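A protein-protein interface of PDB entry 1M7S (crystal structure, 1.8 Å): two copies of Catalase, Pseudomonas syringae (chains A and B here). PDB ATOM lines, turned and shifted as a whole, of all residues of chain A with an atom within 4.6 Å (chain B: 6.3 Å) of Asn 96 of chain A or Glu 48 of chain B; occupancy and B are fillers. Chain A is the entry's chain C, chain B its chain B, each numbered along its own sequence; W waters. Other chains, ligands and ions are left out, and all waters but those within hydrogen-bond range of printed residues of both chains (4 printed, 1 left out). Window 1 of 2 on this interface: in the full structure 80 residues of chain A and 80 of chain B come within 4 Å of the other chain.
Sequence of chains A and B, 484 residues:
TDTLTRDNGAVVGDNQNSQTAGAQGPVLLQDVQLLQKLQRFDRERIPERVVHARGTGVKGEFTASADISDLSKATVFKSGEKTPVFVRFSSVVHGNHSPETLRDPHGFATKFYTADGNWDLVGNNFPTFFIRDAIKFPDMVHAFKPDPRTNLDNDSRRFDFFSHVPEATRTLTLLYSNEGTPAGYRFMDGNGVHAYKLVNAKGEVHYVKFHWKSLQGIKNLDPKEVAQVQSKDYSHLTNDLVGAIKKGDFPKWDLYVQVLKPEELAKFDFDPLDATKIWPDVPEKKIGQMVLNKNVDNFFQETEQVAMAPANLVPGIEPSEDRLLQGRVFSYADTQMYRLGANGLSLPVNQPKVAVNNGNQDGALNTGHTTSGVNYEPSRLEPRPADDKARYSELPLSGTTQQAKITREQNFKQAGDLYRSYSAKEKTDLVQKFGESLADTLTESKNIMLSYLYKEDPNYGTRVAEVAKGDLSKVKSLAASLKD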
ATOM      1  N   ARG A  45      10.200  21.885 -13.337  1.00  0.00           N
ATOM      2  CA  ARG A  45       8.774  22.098 -13.647  1.00  0.00           C
ATOM      3  C   ARG A  45       8.486  22.245 -15.129  1.00  0.00           C
ATOM      4  O   ARG A  45       9.341  22.784 -15.851  1.00  0.00           O
ATOM      5  CB  ARG A  45       8.329  23.411 -12.964  1.00  0.00           C
ATOM      6  CG  ARG A  45       8.553  23.462 -11.438  1.00  0.00           C
ATOM      7  CD  ARG A  45       7.441  22.676 -10.655  1.00  0.00           C
ATOM      8  NE  ARG A  45       7.967  22.530  -9.273  1.00  0.00           N
ATOM      9  CZ  ARG A  45       8.692  21.613  -8.689  1.00  0.00           C
ATOM     10  NH1 ARG A  45       9.070  20.486  -9.234  1.00  0.00           N
ATOM     11  NH2 ARG A  45       9.106  21.775  -7.432  1.00  0.00           N
ATOM     12  N   GLU A  48       1.742  23.376 -16.590  1.00  0.00           N
ATOM     13  CA  GLU A  48       0.634  22.515 -16.178  1.00  0.00           C
ATOM     14  C   GLU A  48      -0.349  22.481 -17.353  1.00  0.00           C
ATOM     15  O   GLU A  48      -0.391  23.398 -18.167  1.00  0.00           O
ATOM     16  CB  GLU A  48      -0.056  23.035 -14.898  1.00  0.00           C
ATOM     17  CG  GLU A  48      -0.822  24.336 -15.050  1.00  0.00           C
ATOM     18  CD  GLU A  48      -1.431  24.892 -13.760  1.00  0.00           C
ATOM     19  OE1 GLU A  48      -1.104  24.510 -12.601  1.00  0.00           O
ATOM     20  OE2 GLU A  48      -2.295  25.807 -13.865  1.00  0.00           O
ATOM     21  N   ALA A  53      -5.666  20.836 -14.702  1.00  0.00           N
ATOM     22  CA  ALA A  53      -4.283  20.740 -14.157  1.00  0.00           C
ATOM     23  C   ALA A  53      -4.177  19.895 -12.902  1.00  0.00           C
ATOM     24  O   ALA A  53      -3.181  19.174 -12.647  1.00  0.00           O
ATOM     25  CB  ALA A  53      -3.752  22.135 -13.883  1.00  0.00           C
ATOM     26  N   ARG A  54      -5.244  20.034 -12.099  1.00  0.00           N
ATOM     27  CA  ARG A  54      -5.281  19.306 -10.807  1.00  0.00           C
ATOM     28  C   ARG A  54      -5.781  17.899 -11.034  1.00  0.00           C
ATOM     29  O   ARG A  54      -6.978  17.777 -11.380  1.00  0.00           O
ATOM     30  CB  ARG A  54      -6.240  20.087  -9.893  1.00  0.00           C
ATOM     31  CG  ARG A  54      -6.495  19.424  -8.557  1.00  0.00           C
ATOM     32  CD  ARG A  54      -5.207  19.125  -7.802  1.00  0.00           C
ATOM     33  NE  ARG A  54      -5.276  19.487  -6.385  1.00  0.00           N
ATOM     34  CZ  ARG A  54      -4.701  18.833  -5.389  1.00  0.00           C
ATOM     35  NH1 ARG A  54      -4.877  19.280  -4.149  1.00  0.00           N
ATOM     36  NH2 ARG A  54      -4.001  17.747  -5.588  1.00  0.00           N
ATOM     37  N   HIS A  94      -9.045  25.163 -11.895  1.00  0.00           N
ATOM     38  CA  HIS A  94      -7.952  25.689 -11.079  1.00  0.00           C
ATOM     39  C   HIS A  94      -6.638  24.946 -11.203  1.00  0.00           C
ATOM     40  O   HIS A  94      -6.535  23.855 -11.759  1.00  0.00           O
ATOM     41  CB  HIS A  94      -8.427  25.828  -9.609  1.00  0.00           C
ATOM     42  CG  HIS A  94      -9.461  26.914  -9.478  1.00  0.00           C
ATOM     43  ND1 HIS A  94     -10.818  26.662  -9.639  1.00  0.00           N
ATOM     44  CD2 HIS A  94      -9.335  28.239  -9.214  1.00  0.00           C
ATOM     45  CE1 HIS A  94     -11.476  27.787  -9.467  1.00  0.00           C
ATOM     46  NE2 HIS A  94     -10.613  28.771  -9.212  1.00  0.00           N
ATOM     47  N   GLY A  95      -5.599  25.554 -10.634  1.00  0.00           N
ATOM     48  CA  GLY A  95      -4.240  25.086 -10.636  1.00  0.00           C
ATOM     49  C   GLY A  95      -3.991  23.749  -9.986  1.00  0.00           C
ATOM     50  O   GLY A  95      -4.798  23.176  -9.264  1.00  0.00           O
ATOM     51  N   ASN A  96      -2.810  23.202 -10.233  1.00  0.00           N
ATOM     52  CA  ASN A  96      -2.370  21.905  -9.765  1.00  0.00           C
ATOM     53  C   ASN A  96      -2.424  21.627  -8.275  1.00  0.00           C
ATOM     54  O   ASN A  96      -2.490  20.406  -8.004  1.00  0.00           O
ATOM     55  CB  ASN A  96      -0.959  21.650 -10.345  1.00  0.00           C
ATOM     56  CG  ASN A  96       0.005  22.694  -9.798  1.00  0.00           C
ATOM     57  OD1 ASN A  96       0.195  22.791  -8.584  1.00  0.00           O
ATOM     58  ND2 ASN A  96       0.590  23.463 -10.709  1.00  0.00           N
ATOM     59  N   HIS A  97      -2.392  22.562  -7.322  1.00  0.00           N
ATOM     60  CA  HIS A  97      -2.583  22.195  -5.916  1.00  0.00           C
ATOM     61  C   HIS A  97      -3.832  22.869  -5.317  1.00  0.00           C
ATOM     62  O   HIS A  97      -3.993  23.100  -4.105  1.00  0.00           O
ATOM     63  CB  HIS A  97      -1.429  22.446  -4.952  1.00  0.00           C
ATOM     64  CG  HIS A  97      -0.294  21.463  -4.967  1.00  0.00           C
ATOM     65  ND1 HIS A  97       1.016  21.856  -4.758  1.00  0.00           N
ATOM     66  CD2 HIS A  97      -0.226  20.132  -5.198  1.00  0.00           C
ATOM     67  CE1 HIS A  97       1.815  20.817  -4.844  1.00  0.00           C
ATOM     68  NE2 HIS A  97       1.084  19.752  -5.126  1.00  0.00           N
ATOM     69  N   SER A  98      -4.750  23.218  -6.211  1.00  0.00           N
ATOM     70  CA  SER A  98      -6.007  23.841  -5.789  1.00  0.00           C
ATOM     71  C   SER A  98      -6.837  22.830  -5.002  1.00  0.00           C
ATOM     72  O   SER A  98      -6.759  21.609  -5.147  1.00  0.00           O
ATOM     73  CB  SER A  98      -6.741  24.301  -7.057  1.00  0.00           C
ATOM     74  OG  SER A  98      -7.018  23.138  -7.840  1.00  0.00           O
ATOM     75  N   ILE B  46       3.109  28.604 -18.747  1.00  0.00           N
ATOM     76  CA  ILE B  46       4.592  28.457 -18.728  1.00  0.00           C
ATOM     77  C   ILE B  46       4.828  27.698 -17.421  1.00  0.00           C
ATOM     78  O   ILE B  46       3.924  27.580 -16.553  1.00  0.00           O
ATOM     79  CB  ILE B  46       5.289  29.805 -18.810  1.00  0.00           C
ATOM     80  CG1 ILE B  46       4.997  30.687 -17.558  1.00  0.00           C
ATOM     81  CG2 ILE B  46       4.863  30.644 -20.041  1.00  0.00           C
ATOM     82  CD1 ILE B  46       5.945  31.912 -17.587  1.00  0.00           C
ATOM     83  N   PRO B  47       5.997  27.184 -17.196  1.00  0.00           N
ATOM     84  CA  PRO B  47       6.319  26.444 -15.977  1.00  0.00           C
ATOM     85  C   PRO B  47       6.164  27.345 -14.743  1.00  0.00           C
ATOM     86  O   PRO B  47       6.509  28.549 -14.823  1.00  0.00           O
ATOM     87  CB  PRO B  47       7.799  26.078 -16.124  1.00  0.00           C
ATOM     88  CG  PRO B  47       7.961  26.033 -17.651  1.00  0.00           C
ATOM     89  CD  PRO B  47       7.149  27.260 -18.116  1.00  0.00           C
ATOM     90  N   GLU B  48       5.568  26.783 -13.670  1.00  0.00           N
ATOM     91  CA  GLU B  48       5.447  27.626 -12.468  1.00  0.00           C
ATOM     92  C   GLU B  48       6.814  27.734 -11.779  1.00  0.00           C
ATOM     93  O   GLU B  48       7.678  26.888 -12.044  1.00  0.00           O
ATOM     94  CB  GLU B  48       4.419  27.103 -11.455  1.00  0.00           C
ATOM     95  CG  GLU B  48       4.683  25.710 -10.923  1.00  0.00           C
ATOM     96  CD  GLU B  48       3.637  25.226  -9.903  1.00  0.00           C
ATOM     97  OE1 GLU B  48       2.510  25.796  -9.823  1.00  0.00           O
ATOM     98  OE2 GLU B  48       3.951  24.226  -9.200  1.00  0.00           O
ATOM     99  N   ARG B  49       6.944  28.713 -10.874  1.00  0.00           N
ATOM    100  CA  ARG B  49       8.238  28.779 -10.147  1.00  0.00           C
ATOM    101  C   ARG B  49       8.473  27.454  -9.435  1.00  0.00           C
ATOM    102  O   ARG B  49       7.555  26.825  -8.876  1.00  0.00           O
ATOM    103  CB  ARG B  49       8.270  29.927  -9.144  1.00  0.00           C
ATOM    104  CG  ARG B  49       8.193  31.320  -9.767  1.00  0.00           C
ATOM    105  CD  ARG B  49       7.714  32.333  -8.723  1.00  0.00           C
ATOM    106  NE  ARG B  49       7.846  33.684  -9.236  1.00  0.00           N
ATOM    107  CZ  ARG B  49       7.182  34.247 -10.216  1.00  0.00           C
ATOM    108  NH1 ARG B  49       6.183  33.599 -10.808  1.00  0.00           N
ATOM    109  NH2 ARG B  49       7.470  35.470 -10.596  1.00  0.00           N
ATOM    110  N   VAL B  50       9.724  27.008  -9.383  1.00  0.00           N
ATOM    111  CA  VAL B  50      10.038  25.741  -8.739  1.00  0.00           C
ATOM    112  C   VAL B  50       9.686  25.774  -7.236  1.00  0.00           C
ATOM    113  O   VAL B  50       9.308  24.759  -6.651  1.00  0.00           O
ATOM    114  CB  VAL B  50      11.484  25.332  -9.067  1.00  0.00           C
ATOM    115  CG1 VAL B  50      12.516  26.282  -8.463  1.00  0.00           C
ATOM    116  CG2 VAL B  50      11.666  23.863  -8.658  1.00  0.00           C
ATOM    117  N   VAL B  51       9.873  26.914  -6.619  1.00  0.00           N
ATOM    118  CA  VAL B  51       9.447  27.198  -5.255  1.00  0.00           C
ATOM    119  C   VAL B  51       8.796  28.562  -5.310  1.00  0.00           C
ATOM    120  O   VAL B  51       9.047  29.399  -6.202  1.00  0.00           O
ATOM    121  CB  VAL B  51      10.533  27.102  -4.174  1.00  0.00           C
ATOM    122  CG1 VAL B  51      10.937  25.651  -3.916  1.00  0.00           C
ATOM    123  CG2 VAL B  51      11.720  27.961  -4.557  1.00  0.00           C
ATOM    124  N   ALA B  53       5.670  29.278  -6.040  1.00  0.00           N
ATOM    125  CA  ALA B  53       4.768  29.331  -7.184  1.00  0.00           C
ATOM    126  C   ALA B  53       3.505  30.156  -6.942  1.00  0.00           C
ATOM    127  O   ALA B  53       2.990  30.930  -7.772  1.00  0.00           O
ATOM    128  CB  ALA B  53       4.384  27.880  -7.523  1.00  0.00           C
ATOM    129  N   ARG B  54       3.036  30.077  -5.695  1.00  0.00           N
ATOM    130  CA  ARG B  54       1.842  30.825  -5.275  1.00  0.00           C
ATOM    131  C   ARG B  54       2.237  32.201  -4.794  1.00  0.00           C
ATOM    132  O   ARG B  54       2.846  32.301  -3.721  1.00  0.00           O
ATOM    133  CB  ARG B  54       1.156  30.002  -4.184  1.00  0.00           C
ATOM    134  CG  ARG B  54      -0.098  30.650  -3.588  1.00  0.00           C
ATOM    135  CD  ARG B  54      -1.215  30.636  -4.611  1.00  0.00           C
ATOM    136  NE  ARG B  54      -2.507  30.239  -4.058  1.00  0.00           N
ATOM    137  CZ  ARG B  54      -3.634  30.895  -4.350  1.00  0.00           C
ATOM    138  NH1 ARG B  54      -4.743  30.462  -3.776  1.00  0.00           N
ATOM    139  NH2 ARG B  54      -3.613  31.940  -5.163  1.00  0.00           N
ATOM    140  N   HIS B  94       3.850  24.833  -1.976  1.00  0.00           N
ATOM    141  CA  HIS B  94       2.818  24.318  -2.877  1.00  0.00           C
ATOM    142  C   HIS B  94       2.573  25.116  -4.153  1.00  0.00           C
ATOM    143  O   HIS B  94       2.977  26.255  -4.374  1.00  0.00           O
ATOM    144  CB  HIS B  94       1.527  24.101  -2.067  1.00  0.00           C
ATOM    145  CG  HIS B  94       1.692  23.028  -1.027  1.00  0.00           C
ATOM    146  ND1 HIS B  94       2.049  23.309   0.273  1.00  0.00           N
ATOM    147  CD2 HIS B  94       1.594  21.682  -1.104  1.00  0.00           C
ATOM    148  CE1 HIS B  94       2.148  22.191   0.947  1.00  0.00           C
ATOM    149  NE2 HIS B  94       1.846  21.186   0.148  1.00  0.00           N
ATOM    150  N   GLY B  95       1.991  24.428  -5.135  1.00  0.00           N
ATOM    151  CA  GLY B  95       1.754  24.940  -6.468  1.00  0.00           C
ATOM    152  C   GLY B  95       0.777  26.080  -6.536  1.00  0.00           C
ATOM    153  O   GLY B  95       0.211  26.486  -5.529  1.00  0.00           O
ATOM    154  N   ASN B  96       0.559  26.625  -7.738  1.00  0.00           N
ATOM    155  CA  ASN B  96      -0.377  27.745  -7.870  1.00  0.00           C
ATOM    156  C   ASN B  96      -1.775  27.272  -7.492  1.00  0.00           C
ATOM    157  O   ASN B  96      -2.133  26.092  -7.494  1.00  0.00           O
ATOM    158  CB  ASN B  96      -0.329  28.360  -9.259  1.00  0.00           C
ATOM    159  CG  ASN B  96      -0.348  27.314 -10.352  1.00  0.00           C
ATOM    160  OD1 ASN B  96      -1.112  26.352 -10.329  1.00  0.00           O
ATOM    161  ND2 ASN B  96       0.546  27.520 -11.317  1.00  0.00           N
ATOM    162  N   HIS B  97      -2.536  28.230  -6.969  1.00  0.00           N
ATOM    163  CA  HIS B  97      -3.858  27.983  -6.435  1.00  0.00           C
ATOM    164  C   HIS B  97      -3.854  27.098  -5.218  1.00  0.00           C
ATOM    165  O   HIS B  97      -4.975  26.741  -4.817  1.00  0.00           O
ATOM    166  CB  HIS B  97      -4.772  27.378  -7.490  1.00  0.00           C
ATOM    167  CG  HIS B  97      -5.098  28.390  -8.548  1.00  0.00           C
ATOM    168  ND1 HIS B  97      -5.385  28.050  -9.851  1.00  0.00           N
ATOM    169  CD2 HIS B  97      -5.150  29.748  -8.500  1.00  0.00           C
ATOM    170  CE1 HIS B  97      -5.617  29.159 -10.545  1.00  0.00           C
ATOM    171  NE2 HIS B  97      -5.472  30.193  -9.743  1.00  0.00           N
ATOM    172  N   LYS B 145       8.449  19.065  -0.046  1.00  0.00           N
ATOM    173  CA  LYS B 145       7.303  18.963  -0.941  1.00  0.00           C
ATOM    174  C   LYS B 145       6.538  17.683  -0.690  1.00  0.00           C
ATOM    175  O   LYS B 145       7.106  16.672  -0.245  1.00  0.00           O
ATOM    176  CB  LYS B 145       7.895  18.871  -2.376  1.00  0.00           C
ATOM    177  CG  LYS B 145       8.564  20.126  -2.911  1.00  0.00           C
ATOM    178  CD  LYS B 145       7.537  21.092  -3.500  1.00  0.00           C
ATOM    179  CE  LYS B 145       8.171  22.211  -4.318  1.00  0.00           C
ATOM    180  NZ  LYS B 145       7.170  23.087  -4.991  1.00  0.00           N
ATOM    181  N   ASN B 151       1.801  12.806  -4.661  1.00  0.00           N
ATOM    182  CA  ASN B 151       1.491  14.222  -4.649  1.00  0.00           C
ATOM    183  C   ASN B 151       0.686  14.567  -3.385  1.00  0.00           C
ATOM    184  O   ASN B 151       0.006  15.590  -3.381  1.00  0.00           O
ATOM    185  CB  ASN B 151       0.724  14.610  -5.907  1.00  0.00           C
ATOM    186  CG  ASN B 151       0.603  16.070  -6.194  1.00  0.00           C
ATOM    187  OD1 ASN B 151       1.550  16.853  -6.071  1.00  0.00           O
ATOM    188  ND2 ASN B 151      -0.561  16.556  -6.598  1.00  0.00           N
ATOM    189  N   GLU B 304       3.265  37.028 -12.736  1.00  0.00           N
ATOM    190  CA  GLU B 304       3.776  35.699 -13.066  1.00  0.00           C
ATOM    191  C   GLU B 304       5.153  35.849 -13.742  1.00  0.00           C
ATOM    192  O   GLU B 304       6.039  35.046 -13.492  1.00  0.00           O
ATOM    193  CB  GLU B 304       2.811  34.935 -13.970  1.00  0.00           C
ATOM    194  CG  GLU B 304       3.236  33.473 -14.152  1.00  0.00           C
ATOM    195  CD  GLU B 304       3.208  32.692 -12.855  1.00  0.00           C
ATOM    196  OE1 GLU B 304       3.920  31.689 -12.681  1.00  0.00           O
ATOM    197  OE2 GLU B 304       2.424  33.082 -11.933  1.00  0.00           O
ATOM    198  N   ARG B 339      12.492  29.319 -17.139  1.00  0.00           N
ATOM    199  CA  ARG B 339      11.072  29.614 -16.921  1.00  0.00           C
ATOM    200  C   ARG B 339      10.590  30.716 -17.832  1.00  0.00           C
ATOM    201  O   ARG B 339       9.423  30.698 -18.272  1.00  0.00           O
ATOM    202  CB  ARG B 339      10.895  30.011 -15.430  1.00  0.00           C
ATOM    203  CG  ARG B 339       9.445  30.301 -15.043  1.00  0.00           C
ATOM    204  CD  ARG B 339       9.294  30.532 -13.552  1.00  0.00           C
ATOM    205  NE  ARG B 339       9.861  31.752 -12.998  1.00  0.00           N
ATOM    206  CZ  ARG B 339       9.434  33.003 -13.055  1.00  0.00           C
ATOM    207  NH1 ARG B 339      10.097  34.002 -12.433  1.00  0.00           N
ATOM    208  NH2 ARG B 339       8.308  33.288 -13.722  1.00  0.00           N
HETATM  209  O   HOH W   1       2.269  25.780 -15.166  1.00  0.00           O
HETATM  210  O   HOH W   2       3.300  22.047  -8.023  1.00  0.00           O
HETATM  211  O   HOH W   3       6.032  20.876  -6.531  1.00  0.00           O
HETATM  212  O   HOH W   4      -3.411  15.122  -7.101  1.00  0.00           O
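OE1 of Glu 48 of chain A sits close to OD1 of Asn 96 of chain B, 2.9 Å away.
The side-chain amide oxygen (OD1) of Asn 96 of chain B is in hydrogen-bond range of the side-chain amide nitrogen (ND2) of Asn 96 of chain A.
N of Gly 95 of chain A sits at hydrogen-bond distance from ND1 of His 97 of chain B (2.6 Å).
The guanidinium group (NH2) of Arg 45 of chain A sits at hydrogen-bond distance from the backbone carbonyl oxygen (O) of Val 50 of chain B, at 3.1 Å.
The side-chain amino group (NZ) of Lys 145 of chain B sits close to the guanidinium group (NH2) of Arg 45 of chain A (3.4 Å).
ND2 of Asn 96 of chain A sits at hydrogen-bond distance from OE1 of Glu 48 of chain B (3.1 Å).
N of Gly 95 of chain B lies within hydrogen-bond range of ND1 of His 97 of chain A (2.8 Å).
A ring nitrogen (NE2) of His 97 of chain A sits at hydrogen-bond distance from the side-chain amide oxygen (OD1) of Asn 151 of chain B (3.1 Å).
The backbone NH (N) of Asn 96 of chain B lies within hydrogen-bond range of the side-chain carboxylate (OE1) of Glu 48 of chain B (3.0 Å).
O of Val 50 of chain B sits at hydrogen-bond distance from NZ of Lys 145 of chain B (3.2 Å).
The backbone carbonyl oxygen (O) of Asn 96 of chain A sits close to the guanidinium group (NE) of Arg 54 of chain A (3.4 Å).
O of Gly 95 of chain A is in hydrogen-bond range of OG of Ser 98 of chain A, at 2.6 Å.
The guanidinium group (NE) of Arg 54 of chain A lies within hydrogen-bond range of the backbone carbonyl oxygen (O) of Ser 98 of chain A, 2.9 Å away.
OE1 of Glu 48 of chain A is in hydrogen-bond range of ND2 of Asn 96 of chain A (2.7 Å).
Among the printed residues, merely in contact across the chains: Arg 45 of chain A with Pro 47 of chain B (3.6 Å), Arg 45 of chain A with Glu 48 of chain B (3.6 Å), Arg 54 of chain A with Asn 151 of chain B (3.8 Å), His 94 of chain A with His 97 of chain B (3.6 Å), Gly 95 of chain A with Asn 96 of chain B (3.4 Å), Asn 96 of chain A with Gly 95 of chain B (3.4 Å), His 97 of chain A with His 94 of chain B (3.5 Å), His 97 of chain A with Asn 96 of chain B (3.5 Å), His 97 of chain A with His 97 of chain B (3.8 Å) and Ser 98 of chain A with His 97 of chain B (3.2 Å).
Of the printed residues of chain B, Asn 96 of chain A touches Glu 48, Gly 95 and Asn 96.
Of the printed residues of chain B, His 94 of chain A touches His 97 (3.6 Å).
Of the printed residues of chain A, His 94 of chain B touches His 97 (3.5 Å).
Of the printed residues of chain B, His 97 of chain A touches His 94 (3.5 Å), Gly 95 (2.8 Å), Asn 96 (3.5 Å), His 97 (3.8 Å) and Asn 151 (3.1 Å).
Of the printed residues of chain A, His 97 of chain B touches His 94 (3.6 Å), Gly 95 (2.6 Å), His 97 (3.8 Å) and Ser 98 (3.2 Å).
Printed residues of chain A within 4 Å of Lys 145 of chain B: Arg 45.
Arg 49 of chain B touches none of the printed residues of chain A.
The nearest printed residue of chain B that does not touch Asn 96 of chain A is Asn 151 of chain B (4.5 Å).
The nearest printed residue of chain A that does not touch Glu 48 of chain B is Glu 48 of chain A (4.7 Å).
Of the 16 printed residues of chain B, 9 touch a printed residue of chain A.
Printed residues of chain B that touch a printed residue of chain A: Pro 47, Glu 48, Val 50, His 94, Gly 95, Asn 96, His 97, Lys 145 and Asn 151.
Hydrophobic or aromatic side chains of chain B that line the printed part of chain A: Pro 47, Val 50, His 94 and His 97.
Among the printed residues, 18 pairs touch across the chains.
Among the printed residues, no Asp or Glu carboxylate lies within 4 Å of a Lys or Arg side-chain nitrogen of the other chain.
His 94 of chain A touches His 97 of chain B, and with the chains exchanged His 97 of chain A touches His 94 of chain B.
Gly 95 of chain A touches Asn 96 of chain B, and with the chains exchanged Asn 96 of chain A touches Gly 95 of chain B.
His 97 of chain A touches Asn 96 of chain B, but with the chains exchanged Asn 96 of chain A does not touch His 97 of chain B (5.4 Å).
His 97 of chain B touches its own counterpart, His 97 of chain A.
Of the 18 pairs that touch across the chains among the printed residues, 10 have their exchanged pair printed and touching as well.
Water W2 lies within hydrogen-bond range of OE2 of Glu 48 of chain B (2.6 Å) and OD1 of Asn 96 of chain A (3.2 Å).
Water W1 lies within hydrogen-bond range of O of Ile 46 of chain B (2.8 Å) and N of Glu 48 of chain A (2.8 Å).
Water W3 lies within hydrogen-bond range of the side-chain amino group of Lys 145 of chain B and the guanidinium group of Arg 45 of chain A.
Water W4 lies within hydrogen-bond range of the guanidinium group (NH2) of Arg 54 of chain A (3.1 Å) and the side-chain amide nitrogen (ND2) of Asn 151 of chain B (3.2 Å).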
